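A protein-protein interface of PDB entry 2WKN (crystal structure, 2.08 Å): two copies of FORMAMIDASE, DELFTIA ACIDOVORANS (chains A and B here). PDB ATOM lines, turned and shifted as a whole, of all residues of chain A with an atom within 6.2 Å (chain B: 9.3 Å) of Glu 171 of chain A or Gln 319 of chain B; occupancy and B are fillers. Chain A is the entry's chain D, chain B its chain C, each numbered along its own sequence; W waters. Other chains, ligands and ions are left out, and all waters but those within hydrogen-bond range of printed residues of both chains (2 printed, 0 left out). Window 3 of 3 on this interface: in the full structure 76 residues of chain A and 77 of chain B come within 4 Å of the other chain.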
ATOM      1  N   SER A 166     -21.869 -29.119 -22.865  1.00  0.00           N
ATOM      2  CA  SER A 166     -21.775 -28.146 -21.765  1.00  0.00           C
ATOM      3  C   SER A 166     -20.328 -27.818 -21.440  1.00  0.00           C
ATOM      4  O   SER A 166     -19.974 -26.632 -21.308  1.00  0.00           O
ATOM      5  CB  SER A 166     -22.455 -28.657 -20.498  1.00  0.00           C
ATOM      6  OG  SER A 166     -23.788 -29.064 -20.759  1.00  0.00           O
ATOM      7  N   TRP A 167     -19.492 -28.861 -21.330  1.00  0.00           N
ATOM      8  CA  TRP A 167     -18.082 -28.674 -20.994  1.00  0.00           C
ATOM      9  C   TRP A 167     -17.406 -27.730 -21.989  1.00  0.00           C
ATOM     10  O   TRP A 167     -16.808 -26.726 -21.603  1.00  0.00           O
ATOM     11  CB  TRP A 167     -17.311 -30.014 -20.908  1.00  0.00           C
ATOM     12  CG  TRP A 167     -17.782 -30.989 -19.842  1.00  0.00           C
ATOM     13  CD1 TRP A 167     -18.712 -30.768 -18.870  1.00  0.00           C
ATOM     14  CD2 TRP A 167     -17.304 -32.325 -19.638  1.00  0.00           C
ATOM     15  NE1 TRP A 167     -18.867 -31.891 -18.092  1.00  0.00           N
ATOM     16  CE2 TRP A 167     -18.005 -32.857 -18.534  1.00  0.00           C
ATOM     17  CE3 TRP A 167     -16.355 -33.125 -20.285  1.00  0.00           C
ATOM     18  CZ2 TRP A 167     -17.787 -34.156 -18.058  1.00  0.00           C
ATOM     19  CZ3 TRP A 167     -16.138 -34.428 -19.805  1.00  0.00           C
ATOM     20  CH2 TRP A 167     -16.851 -34.921 -18.703  1.00  0.00           C
ATOM     21  N   ASN A 168     -17.490 -28.065 -23.270  1.00  0.00           N
ATOM     22  CA  ASN A 168     -16.878 -27.242 -24.310  1.00  0.00           C
ATOM     23  C   ASN A 168     -17.427 -25.803 -24.315  1.00  0.00           C
ATOM     24  O   ASN A 168     -16.654 -24.853 -24.363  1.00  0.00           O
ATOM     25  CB  ASN A 168     -17.016 -27.907 -25.689  1.00  0.00           C
ATOM     26  CG  ASN A 168     -16.283 -29.242 -25.772  1.00  0.00           C
ATOM     27  OD1 ASN A 168     -15.340 -29.496 -25.017  1.00  0.00           O
ATOM     28  ND2 ASN A 168     -16.723 -30.103 -26.681  1.00  0.00           N
ATOM     29  N   GLU A 169     -18.749 -25.653 -24.210  1.00  0.00           N
ATOM     30  CA  GLU A 169     -19.374 -24.334 -24.210  1.00  0.00           C
ATOM     31  C   GLU A 169     -18.883 -23.405 -23.087  1.00  0.00           C
ATOM     32  O   GLU A 169     -18.436 -22.273 -23.352  1.00  0.00           O
ATOM     33  CB  GLU A 169     -20.891 -24.461 -24.146  1.00  0.00           C
ATOM     34  CG  GLU A 169     -21.632 -23.146 -24.359  1.00  0.00           C
ATOM     35  CD  GLU A 169     -23.132 -23.287 -24.130  1.00  0.00           C
ATOM     36  OE1 GLU A 169     -23.874 -23.460 -25.124  1.00  0.00           O
ATOM     37  OE2 GLU A 169     -23.573 -23.245 -22.958  1.00  0.00           O
ATOM     38  N   ARG A 170     -18.966 -23.877 -21.840  1.00  0.00           N
ATOM     39  CA  ARG A 170     -18.553 -23.060 -20.706  1.00  0.00           C
ATOM     40  C   ARG A 170     -17.031 -22.805 -20.678  1.00  0.00           C
ATOM     41  O   ARG A 170     -16.591 -21.732 -20.271  1.00  0.00           O
ATOM     42  CB  ARG A 170     -19.071 -23.642 -19.381  1.00  0.00           C
ATOM     43  CG  ARG A 170     -18.364 -24.897 -18.886  1.00  0.00           C
ATOM     44  CD  ARG A 170     -19.128 -25.603 -17.754  1.00  0.00           C
ATOM     45  NE  ARG A 170     -18.313 -26.646 -17.134  1.00  0.00           N
ATOM     46  CZ  ARG A 170     -18.787 -27.732 -16.519  1.00  0.00           C
ATOM     47  NH1 ARG A 170     -20.098 -27.962 -16.432  1.00  0.00           N
ATOM     48  NH2 ARG A 170     -17.933 -28.610 -15.992  1.00  0.00           N
ATOM     49  N   GLU A 171     -16.248 -23.774 -21.146  1.00  0.00           N
ATOM     50  CA  GLU A 171     -14.784 -23.670 -21.114  1.00  0.00           C
ATOM     51  C   GLU A 171     -14.213 -22.815 -22.238  1.00  0.00           C
ATOM     52  O   GLU A 171     -13.273 -22.037 -22.011  1.00  0.00           O
ATOM     53  CB  GLU A 171     -14.124 -25.060 -21.100  1.00  0.00           C
ATOM     54  CG  GLU A 171     -14.211 -25.765 -19.738  1.00  0.00           C
ATOM     55  CD  GLU A 171     -13.922 -27.261 -19.798  1.00  0.00           C
ATOM     56  OE1 GLU A 171     -13.016 -27.644 -20.578  1.00  0.00           O
ATOM     57  OE2 GLU A 171     -14.603 -28.037 -19.059  1.00  0.00           O
ATOM     58  N   THR A 172     -14.753 -22.970 -23.446  1.00  0.00           N
ATOM     59  CA  THR A 172     -14.376 -22.070 -24.550  1.00  0.00           C
ATOM     60  C   THR A 172     -14.874 -20.644 -24.259  1.00  0.00           C
ATOM     61  O   THR A 172     -14.172 -19.663 -24.542  1.00  0.00           O
ATOM     62  CB  THR A 172     -14.881 -22.551 -25.928  1.00  0.00           C
ATOM     63  OG1 THR A 172     -16.293 -22.774 -25.876  1.00  0.00           O
ATOM     64  CG2 THR A 172     -14.161 -23.826 -26.367  1.00  0.00           C
ATOM     65  N   GLY A 173     -16.065 -20.545 -23.658  1.00  0.00           N
ATOM     66  CA  GLY A 173     -16.622 -19.264 -23.200  1.00  0.00           C
ATOM     67  C   GLY A 173     -15.681 -18.509 -22.282  1.00  0.00           C
ATOM     68  O   GLY A 173     -15.530 -17.292 -22.403  1.00  0.00           O
ATOM     69  N   LEU A 174     -15.031 -19.240 -21.375  1.00  0.00           N
ATOM     70  CA  LEU A 174     -14.077 -18.654 -20.432  1.00  0.00           C
ATOM     71  C   LEU A 174     -12.752 -18.238 -21.089  1.00  0.00           C
ATOM     72  O   LEU A 174     -12.177 -17.197 -20.734  1.00  0.00           O
ATOM     73  CB  LEU A 174     -13.830 -19.608 -19.254  1.00  0.00           C
ATOM     74  CG  LEU A 174     -12.813 -19.194 -18.187  1.00  0.00           C
ATOM     75  CD1 LEU A 174     -13.394 -18.139 -17.257  1.00  0.00           C
ATOM     76  CD2 LEU A 174     -12.351 -20.412 -17.394  1.00  0.00           C
ATOM     77  N   ILE A 175     -12.262 -19.039 -22.034  1.00  0.00           N
ATOM     78  CA  ILE A 175     -11.076 -18.655 -22.820  1.00  0.00           C
ATOM     79  C   ILE A 175     -11.347 -17.336 -23.571  1.00  0.00           C
ATOM     80  O   ILE A 175     -10.474 -16.465 -23.640  1.00  0.00           O
ATOM     81  CB  ILE A 175     -10.613 -19.769 -23.801  1.00  0.00           C
ATOM     82  CG1 ILE A 175     -10.220 -21.039 -23.032  1.00  0.00           C
ATOM     83  CG2 ILE A 175      -9.437 -19.287 -24.652  1.00  0.00           C
ATOM     84  CD1 ILE A 175     -10.156 -22.296 -23.891  1.00  0.00           C
ATOM     85  N   ALA A 176     -12.571 -17.196 -24.088  1.00  0.00           N
ATOM     86  CA  ALA A 176     -13.004 -15.994 -24.821  1.00  0.00           C
ATOM     87  C   ALA A 176     -12.838 -14.694 -24.034  1.00  0.00           C
ATOM     88  O   ALA A 176     -12.573 -13.650 -24.627  1.00  0.00           O
ATOM     89  CB  ALA A 176     -14.450 -16.145 -25.311  1.00  0.00           C
ATOM     90  N   ALA A 186      -8.148 -21.974 -19.738  1.00  0.00           N
ATOM     91  CA  ALA A 186      -8.635 -23.326 -20.017  1.00  0.00           C
ATOM     92  C   ALA A 186      -7.951 -23.892 -21.267  1.00  0.00           C
ATOM     93  O   ALA A 186      -7.184 -23.193 -21.931  1.00  0.00           O
ATOM     94  CB  ALA A 186     -10.157 -23.337 -20.177  1.00  0.00           C
ATOM     95  N   ASN A 187      -8.210 -25.155 -21.576  1.00  0.00           N
ATOM     96  CA  ASN A 187      -7.638 -25.762 -22.768  1.00  0.00           C
ATOM     97  C   ASN A 187      -8.769 -26.267 -23.655  1.00  0.00           C
ATOM     98  O   ASN A 187      -9.570 -27.083 -23.211  1.00  0.00           O
ATOM     99  CB  ASN A 187      -6.668 -26.895 -22.406  1.00  0.00           C
ATOM    100  CG  ASN A 187      -5.504 -26.415 -21.553  1.00  0.00           C
ATOM    101  OD1 ASN A 187      -4.571 -25.793 -22.059  1.00  0.00           O
ATOM    102  ND2 ASN A 187      -5.559 -26.692 -20.247  1.00  0.00           N
ATOM    103  N   ALA A 212     -13.048 -33.378 -25.377  1.00  0.00           N
ATOM    104  CA  ALA A 212     -12.591 -32.515 -24.268  1.00  0.00           C
ATOM    105  C   ALA A 212     -11.191 -32.869 -23.765  1.00  0.00           C
ATOM    106  O   ALA A 212     -10.857 -34.034 -23.642  1.00  0.00           O
ATOM    107  CB  ALA A 212     -13.589 -32.540 -23.119  1.00  0.00           C
ATOM    108  N   ARG A 213     -10.372 -31.856 -23.486  1.00  0.00           N
ATOM    109  CA  ARG A 213      -9.127 -32.089 -22.778  1.00  0.00           C
ATOM    110  C   ARG A 213      -9.391 -32.747 -21.421  1.00  0.00           C
ATOM    111  O   ARG A 213     -10.408 -32.471 -20.798  1.00  0.00           O
ATOM    112  CB  ARG A 213      -8.348 -30.788 -22.595  1.00  0.00           C
ATOM    113  CG  ARG A 213      -7.943 -30.111 -23.901  1.00  0.00           C
ATOM    114  CD  ARG A 213      -7.077 -31.012 -24.756  1.00  0.00           C
ATOM    115  NE  ARG A 213      -5.959 -31.580 -24.012  1.00  0.00           N
ATOM    116  CZ  ARG A 213      -4.864 -30.906 -23.659  1.00  0.00           C
ATOM    117  NH1 ARG A 213      -4.732 -29.620 -23.968  1.00  0.00           N
ATOM    118  NH2 ARG A 213      -3.903 -31.525 -22.969  1.00  0.00           N
ATOM    119  N   PRO A 216      -8.962 -30.701 -16.698  1.00  0.00           N
ATOM    120  CA  PRO A 216      -9.650 -30.330 -15.460  1.00  0.00           C
ATOM    121  C   PRO A 216     -10.583 -31.405 -14.897  1.00  0.00           C
ATOM    122  O   PRO A 216     -11.143 -32.178 -15.672  1.00  0.00           O
ATOM    123  CB  PRO A 216     -10.492 -29.124 -15.892  1.00  0.00           C
ATOM    124  CG  PRO A 216     -10.860 -29.425 -17.393  1.00  0.00           C
ATOM    125  CD  PRO A 216      -9.784 -30.397 -17.898  1.00  0.00           C
ATOM    126  N   PRO A 217     -10.758 -31.442 -13.554  1.00  0.00           N
ATOM    127  CA  PRO A 217     -11.815 -32.243 -12.941  1.00  0.00           C
ATOM    128  C   PRO A 217     -13.164 -31.682 -13.330  1.00  0.00           C
ATOM    129  O   PRO A 217     -13.284 -30.484 -13.540  1.00  0.00           O
ATOM    130  CB  PRO A 217     -11.621 -31.997 -11.440  1.00  0.00           C
ATOM    131  CG  PRO A 217     -10.894 -30.671 -11.371  1.00  0.00           C
ATOM    132  CD  PRO A 217      -9.974 -30.711 -12.544  1.00  0.00           C
ATOM    133  N   ARG A 218     -14.168 -32.544 -13.414  1.00  0.00           N
ATOM    134  CA  ARG A 218     -15.515 -32.113 -13.811  1.00  0.00           C
ATOM    135  C   ARG A 218     -16.503 -33.010 -13.091  1.00  0.00           C
ATOM    136  O   ARG A 218     -16.098 -33.846 -12.266  1.00  0.00           O
ATOM    137  CB  ARG A 218     -15.703 -32.232 -15.329  1.00  0.00           C
ATOM    138  CG  ARG A 218     -14.714 -31.402 -16.178  1.00  0.00           C
ATOM    139  CD  ARG A 218     -15.041 -31.572 -17.652  1.00  0.00           C
ATOM    140  NE  ARG A 218     -14.205 -30.790 -18.562  1.00  0.00           N
ATOM    141  CZ  ARG A 218     -13.145 -31.265 -19.214  1.00  0.00           C
ATOM    142  NH1 ARG A 218     -12.759 -32.530 -19.050  1.00  0.00           N
ATOM    143  NH2 ARG A 218     -12.478 -30.469 -20.052  1.00  0.00           N
ATOM    144  N   ILE B 311     -16.239 -28.647  -7.934  1.00  0.00           N
ATOM    145  CA  ILE B 311     -15.359 -27.970  -8.895  1.00  0.00           C
ATOM    146  C   ILE B 311     -15.825 -26.528  -9.066  1.00  0.00           C
ATOM    147  O   ILE B 311     -16.938 -26.178  -8.677  1.00  0.00           O
ATOM    148  CB  ILE B 311     -15.382 -28.667 -10.308  1.00  0.00           C
ATOM    149  CG1 ILE B 311     -16.816 -28.706 -10.879  1.00  0.00           C
ATOM    150  CG2 ILE B 311     -14.744 -30.070 -10.261  1.00  0.00           C
ATOM    151  CD1 ILE B 311     -16.883 -29.093 -12.325  1.00  0.00           C
ATOM    152  N   SER B 312     -14.983 -25.709  -9.672  1.00  0.00           N
ATOM    153  CA  SER B 312     -15.235 -24.301  -9.846  1.00  0.00           C
ATOM    154  C   SER B 312     -16.302 -23.968 -10.903  1.00  0.00           C
ATOM    155  O   SER B 312     -16.075 -23.137 -11.762  1.00  0.00           O
ATOM    156  CB  SER B 312     -13.926 -23.599 -10.205  1.00  0.00           C
ATOM    157  OG  SER B 312     -12.925 -23.947  -9.291  1.00  0.00           O
ATOM    158  N   VAL B 313     -17.467 -24.606 -10.809  1.00  0.00           N
ATOM    159  CA  VAL B 313     -18.601 -24.303 -11.678  1.00  0.00           C
ATOM    160  C   VAL B 313     -19.794 -24.160 -10.755  1.00  0.00           C
ATOM    161  O   VAL B 313     -20.165 -25.134 -10.101  1.00  0.00           O
ATOM    162  CB  VAL B 313     -18.877 -25.443 -12.697  1.00  0.00           C
ATOM    163  CG1 VAL B 313     -20.216 -25.225 -13.435  1.00  0.00           C
ATOM    164  CG2 VAL B 313     -17.742 -25.596 -13.689  1.00  0.00           C
ATOM    165  N   ASP B 314     -20.410 -22.964 -10.732  1.00  0.00           N
ATOM    166  CA  ASP B 314     -21.428 -22.633  -9.723  1.00  0.00           C
ATOM    167  C   ASP B 314     -22.810 -23.250  -9.944  1.00  0.00           C
ATOM    168  O   ASP B 314     -22.986 -24.064 -10.843  1.00  0.00           O
ATOM    169  CB  ASP B 314     -21.507 -21.120  -9.442  1.00  0.00           C
ATOM    170  CG  ASP B 314     -22.007 -20.293 -10.651  1.00  0.00           C
ATOM    171  OD1 ASP B 314     -22.990 -20.675 -11.332  1.00  0.00           O
ATOM    172  OD2 ASP B 314     -21.399 -19.235 -10.890  1.00  0.00           O
ATOM    173  N   GLU B 315     -23.766 -22.887  -9.089  1.00  0.00           N
ATOM    174  CA  GLU B 315     -25.121 -23.475  -9.107  1.00  0.00           C
ATOM    175  C   GLU B 315     -25.876 -23.150 -10.403  1.00  0.00           C
ATOM    176  O   GLU B 315     -26.812 -23.865 -10.782  1.00  0.00           O
ATOM    177  CB  GLU B 315     -25.960 -22.991  -7.915  1.00  0.00           C
ATOM    178  CG  GLU B 315     -25.417 -23.305  -6.541  1.00  0.00           C
ATOM    179  CD  GLU B 315     -24.530 -22.200  -5.971  1.00  0.00           C
ATOM    180  OE1 GLU B 315     -23.544 -21.821  -6.625  1.00  0.00           O
ATOM    181  OE2 GLU B 315     -24.825 -21.708  -4.856  1.00  0.00           O
ATOM    182  N   LYS B 316     -25.466 -22.070 -11.064  1.00  0.00           N
ATOM    183  CA  LYS B 316     -26.093 -21.645 -12.313  1.00  0.00           C
ATOM    184  C   LYS B 316     -25.431 -22.280 -13.546  1.00  0.00           C
ATOM    185  O   LYS B 316     -25.920 -22.131 -14.671  1.00  0.00           O
ATOM    186  CB  LYS B 316     -26.101 -20.109 -12.419  1.00  0.00           C
ATOM    187  CG  LYS B 316     -26.912 -19.402 -11.325  1.00  0.00           C
ATOM    188  CD  LYS B 316     -28.415 -19.684 -11.445  1.00  0.00           C
ATOM    189  CE  LYS B 316     -29.183 -19.242 -10.198  1.00  0.00           C
ATOM    190  NZ  LYS B 316     -29.076 -17.771  -9.942  1.00  0.00           N
ATOM    191  N   GLY B 317     -24.324 -22.992 -13.325  1.00  0.00           N
ATOM    192  CA  GLY B 317     -23.587 -23.633 -14.409  1.00  0.00           C
ATOM    193  C   GLY B 317     -22.514 -22.744 -15.018  1.00  0.00           C
ATOM    194  O   GLY B 317     -21.899 -23.121 -16.019  1.00  0.00           O
ATOM    195  N   LYS B 318     -22.304 -21.560 -14.434  1.00  0.00           N
ATOM    196  CA  LYS B 318     -21.250 -20.649 -14.890  1.00  0.00           C
ATOM    197  C   LYS B 318     -19.870 -21.192 -14.540  1.00  0.00           C
ATOM    198  O   LYS B 318     -19.706 -21.858 -13.511  1.00  0.00           O
ATOM    199  CB  LYS B 318     -21.400 -19.235 -14.293  1.00  0.00           C
ATOM    200  CG  LYS B 318     -22.818 -18.640 -14.311  1.00  0.00           C
ATOM    201  CD  LYS B 318     -23.376 -18.376 -15.725  1.00  0.00           C
ATOM    202  CE  LYS B 318     -23.083 -16.952 -16.195  1.00  0.00           C
ATOM    203  NZ  LYS B 318     -21.624 -16.744 -16.422  1.00  0.00           N
ATOM    204  N   GLN B 319     -18.887 -20.869 -15.382  1.00  0.00           N
ATOM    205  CA  GLN B 319     -17.540 -21.376 -15.256  1.00  0.00           C
ATOM    206  C   GLN B 319     -16.661 -20.330 -14.596  1.00  0.00           C
ATOM    207  O   GLN B 319     -16.570 -19.209 -15.089  1.00  0.00           O
ATOM    208  CB  GLN B 319     -17.002 -21.748 -16.637  1.00  0.00           C
ATOM    209  CG  GLN B 319     -15.564 -22.245 -16.656  1.00  0.00           C
ATOM    210  CD  GLN B 319     -15.410 -23.634 -16.036  1.00  0.00           C
ATOM    211  OE1 GLN B 319     -16.028 -24.617 -16.476  1.00  0.00           O
ATOM    212  NE2 GLN B 319     -14.602 -23.707 -14.987  1.00  0.00           N
ATOM    213  N   HIS B 320     -16.032 -20.695 -13.474  1.00  0.00           N
ATOM    214  CA  HIS B 320     -15.103 -19.794 -12.806  1.00  0.00           C
ATOM    215  C   HIS B 320     -13.681 -20.239 -13.087  1.00  0.00           C
ATOM    216  O   HIS B 320     -13.474 -21.212 -13.802  1.00  0.00           O
ATOM    217  CB  HIS B 320     -15.391 -19.720 -11.311  1.00  0.00           C
ATOM    218  CG  HIS B 320     -16.713 -19.094 -10.984  1.00  0.00           C
ATOM    219  ND1 HIS B 320     -16.828 -17.858 -10.380  1.00  0.00           N
ATOM    220  CD2 HIS B 320     -17.979 -19.540 -11.178  1.00  0.00           C
ATOM    221  CE1 HIS B 320     -18.109 -17.577 -10.208  1.00  0.00           C
ATOM    222  NE2 HIS B 320     -18.827 -18.583 -10.681  1.00  0.00           N
ATOM    223  N   TYR B 321     -12.706 -19.525 -12.545  1.00  0.00           N
ATOM    224  CA  TYR B 321     -11.310 -19.859 -12.775  1.00  0.00           C
ATOM    225  C   TYR B 321     -10.571 -20.131 -11.470  1.00  0.00           C
ATOM    226  O   TYR B 321     -10.379 -19.222 -10.655  1.00  0.00           O
ATOM    227  CB  TYR B 321     -10.619 -18.735 -13.539  1.00  0.00           C
ATOM    228  CG  TYR B 321      -9.134 -18.937 -13.676  1.00  0.00           C
ATOM    229  CD1 TYR B 321      -8.624 -19.929 -14.522  1.00  0.00           C
ATOM    230  CD2 TYR B 321      -8.240 -18.144 -12.960  1.00  0.00           C
ATOM    231  CE1 TYR B 321      -7.257 -20.125 -14.650  1.00  0.00           C
ATOM    232  CE2 TYR B 321      -6.865 -18.321 -13.082  1.00  0.00           C
ATOM    233  CZ  TYR B 321      -6.382 -19.305 -13.927  1.00  0.00           C
ATOM    234  OH  TYR B 321      -5.040 -19.497 -14.030  1.00  0.00           O
ATOM    235  N   LEU B 322     -10.140 -21.383 -11.299  1.00  0.00           N
ATOM    236  CA  LEU B 322      -9.410 -21.836 -10.090  1.00  0.00           C
ATOM    237  C   LEU B 322     -10.018 -21.237  -8.822  1.00  0.00           C
ATOM    238  O   LEU B 322      -9.319 -20.617  -8.025  1.00  0.00           O
ATOM    239  CB  LEU B 322      -7.909 -21.471 -10.195  1.00  0.00           C
ATOM    240  CG  LEU B 322      -7.025 -22.194 -11.219  1.00  0.00           C
ATOM    241  CD1 LEU B 322      -5.576 -21.651 -11.187  1.00  0.00           C
ATOM    242  CD2 LEU B 322      -7.007 -23.705 -11.019  1.00  0.00           C
ATOM    243  N   ASP B 323     -11.331 -21.382  -8.663  1.00  0.00           N
ATOM    244  CA  ASP B 323     -12.015 -20.757  -7.549  1.00  0.00           C
ATOM    245  C   ASP B 323     -12.369 -21.823  -6.540  1.00  0.00           C
ATOM    246  O   ASP B 323     -13.359 -22.539  -6.725  1.00  0.00           O
ATOM    247  CB  ASP B 323     -13.277 -20.014  -8.012  1.00  0.00           C
ATOM    248  CG  ASP B 323     -13.876 -19.116  -6.915  1.00  0.00           C
ATOM    249  OD1 ASP B 323     -14.102 -19.590  -5.774  1.00  0.00           O
ATOM    250  OD2 ASP B 323     -14.135 -17.927  -7.193  1.00  0.00           O
ATOM    251  N   VAL B 326     -15.938 -21.413  -4.764  1.00  0.00           N
ATOM    252  CA  VAL B 326     -17.053 -21.997  -5.492  1.00  0.00           C
ATOM    253  C   VAL B 326     -17.025 -23.526  -5.479  1.00  0.00           C
ATOM    254  O   VAL B 326     -18.056 -24.165  -5.426  1.00  0.00           O
ATOM    255  CB  VAL B 326     -17.109 -21.494  -6.948  1.00  0.00           C
ATOM    256  CG1 VAL B 326     -18.180 -22.250  -7.724  1.00  0.00           C
ATOM    257  CG2 VAL B 326     -17.389 -19.988  -6.982  1.00  0.00           C
ATOM    258  N   ASP B 367      -5.459 -27.462 -11.910  1.00  0.00           N
ATOM    259  CA  ASP B 367      -5.967 -28.100 -13.113  1.00  0.00           C
ATOM    260  C   ASP B 367      -6.927 -27.178 -13.880  1.00  0.00           C
ATOM    261  O   ASP B 367      -8.116 -27.461 -13.987  1.00  0.00           O
ATOM    262  CB  ASP B 367      -6.634 -29.443 -12.766  1.00  0.00           C
ATOM    263  CG  ASP B 367      -5.631 -30.483 -12.260  1.00  0.00           C
ATOM    264  OD1 ASP B 367      -4.472 -30.495 -12.713  1.00  0.00           O
ATOM    265  OD2 ASP B 367      -6.017 -31.290 -11.391  1.00  0.00           O
ATOM    266  N   VAL B 368      -6.376 -26.073 -14.390  1.00  0.00           N
ATOM    267  CA  VAL B 368      -7.162 -25.013 -15.040  1.00  0.00           C
ATOM    268  C   VAL B 368      -8.244 -25.579 -15.972  1.00  0.00           C
ATOM    269  O   VAL B 368      -7.957 -26.476 -16.777  1.00  0.00           O
ATOM    270  CB  VAL B 368      -6.269 -23.998 -15.792  1.00  0.00           C
ATOM    271  CG1 VAL B 368      -5.328 -23.283 -14.807  1.00  0.00           C
ATOM    272  CG2 VAL B 368      -5.483 -24.677 -16.902  1.00  0.00           C
ATOM    273  N   PRO B 369      -9.497 -25.062 -15.867  1.00  0.00           N
ATOM    274  CA  PRO B 369      -9.940 -23.951 -15.028  1.00  0.00           C
ATOM    275  C   PRO B 369     -10.467 -24.334 -13.648  1.00  0.00           C
ATOM    276  O   PRO B 369     -10.827 -23.438 -12.887  1.00  0.00           O
ATOM    277  CB  PRO B 369     -11.111 -23.378 -15.836  1.00  0.00           C
ATOM    278  CG  PRO B 369     -11.741 -24.581 -16.437  1.00  0.00           C
ATOM    279  CD  PRO B 369     -10.594 -25.524 -16.752  1.00  0.00           C
ATOM    280  N   ASN B 370     -10.555 -25.627 -13.339  1.00  0.00           N
ATOM    281  CA  ASN B 370     -11.231 -26.049 -12.107  1.00  0.00           C
ATOM    282  C   ASN B 370     -10.326 -26.394 -10.929  1.00  0.00           C
ATOM    283  O   ASN B 370      -9.436 -27.243 -11.037  1.00  0.00           O
ATOM    284  CB  ASN B 370     -12.187 -27.209 -12.377  1.00  0.00           C
ATOM    285  CG  ASN B 370     -13.346 -26.816 -13.270  1.00  0.00           C
ATOM    286  OD1 ASN B 370     -13.811 -25.677 -13.226  1.00  0.00           O
ATOM    287  ND2 ASN B 370     -13.828 -27.764 -14.087  1.00  0.00           N
ATOM    288  N   ALA B 371     -10.558 -25.711  -9.810  1.00  0.00           N
ATOM    289  CA  ALA B 371     -10.073 -26.160  -8.510  1.00  0.00           C
ATOM    290  C   ALA B 371     -10.915 -27.348  -8.135  1.00  0.00           C
ATOM    291  O   ALA B 371     -12.053 -27.469  -8.616  1.00  0.00           O
ATOM    292  CB  ALA B 371     -10.222 -25.084  -7.496  1.00  0.00           C
HETATM  293  O   HOH W   1      -7.995 -27.144 -19.508  1.00  0.00           O
HETATM  294  O   HOH W   2     -22.311 -25.697 -17.029  1.00  0.00           O
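Of chain B, only Gln 319 (3.9 Å) comes within 4 Å of Glu 171 of chain A.
Gln 319 of chain B touches just these residues of chain A: Arg 170, Glu 171 and Leu 174.
No residue of chain B comes within 4 Å of Thr 172 of chain A.
Printed residues of chain B within 4 Å of Pro 217 of chain A: Ile 311 (3.6 Å), Asp 367 (3.6 Å) and Asn 370 (2.8 Å).
Of the printed residues of chain B, Arg 218 of chain A touches Ile 311.
Of the printed residues of chain B, Pro 216 of chain A touches Asp 367 (3.5 Å), Val 368 (3.8 Å) and Pro 369 (3.7 Å).
Printed residues of chain A within 4 Å of Asn 370 of chain B: Pro 217 (2.8 Å).
Printed residues of chain B within 4 Å of Asn 187 of chain A: Val 368.
Tyr 321 of chain B touches none of the printed residues of chain A.
The nearest residue of chain B that does not touch Glu 171 of chain A is Pro 369 of chain B (4.3 Å).
The nearest printed residue of chain A that does not touch His 320 of chain B is Arg 170 of chain A (6.9 Å).
Water W1 bridges the side-chain amide nitrogen of Asn 187 of chain A (2.6 Å) and the backbone carbonyl oxygen of Val 368 of chain B (2.8 Å).
Water W2 lies within hydrogen-bond range of the backbone carbonyl oxygen of Gly 317 of chain B (2.8 Å) and the guanidinium group of Arg 170 of chain A (3.2 Å).
NE2 of Gln 319 of chain B lies within hydrogen-bond range of OD1 of Asn 370 of chain B.
O of Pro 369 of chain B is in hydrogen-bond range of N of Leu 322 of chain B (2.7 Å).
The side-chain carboxylate (OE2) of Glu 171 of chain A lies within salt-bridge range of the guanidinium group (NE) of Arg 218 of chain A (2.8 Å).
O of Ser 312 of chain B sits at hydrogen-bond distance from N of His 320 of chain B (3.0 Å).
The guanidinium group of Arg 218 of chain A sits at hydrogen-bond distance from the backbone carbonyl oxygen of Arg 213 of chain A (2.9 Å).
OD2 of Asp 314 of chain B sits at hydrogen-bond distance from NE2 of His 320 of chain B (2.7 Å).
No position is printed for both chains.
Of the 15 pairs that touch across the chains among the printed residues, none has its exchanged pair printed and touching as well.
The side-chain amide nitrogen (ND2) of Asn 370 of chain B sits at hydrogen-bond distance from the backbone carbonyl oxygen (O) of Pro 217 of chain A, 2.8 Å away.
The side-chain amide oxygen of Gln 319 of chain B sits at hydrogen-bond distance from the guanidinium group of Arg 170 of chain A, at 3.1 Å.
Hydrophobic or aromatic side chains of chain A within 4 Å of the printed part of chain B: Leu 174, Pro 216 and Pro 217.
Hydrophobic or aromatic side chains of chain B that line the printed part of chain A: Ile 311, Val 313, Val 368 and Pro 369.
Among the printed residues, 15 pairs touch across the chains.
Among the printed residues, no Asp or Glu carboxylate lies within 4 Å of a Lys or Arg side-chain nitrogen of the other chain.
Arg 170 of chain A touches Val 313 of chain B (NE to CG2, 3.6 Å).
Gln 319 of chain B touches Glu 171 of chain A.
Leu 174 of chain A touches His 320 of chain B (CD2 to O, 3.8 Å).
Pro 369 of chain B touches Leu 174 of chain A (CB to CD2, 3.6 Å).
Val 368 of chain B touches Asn 187 of chain A (CG2 to ND2, 3.9 Å).
CB of Pro 216 of chain A touches O of Asp 367 of chain B, 3.5 Å away.
Val 368 of chain B touches Pro 216 of chain A (O to CB, 3.8 Å).
Pro 217 of chain A touches Ile 311 of chain B (O to CG2, 3.6 Å).
Pro 217 of chain A touches Asp 367 of chain B.
CA of Arg 218 of chain A touches CD1 of Ile 311 of chain B (3.6 Å).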
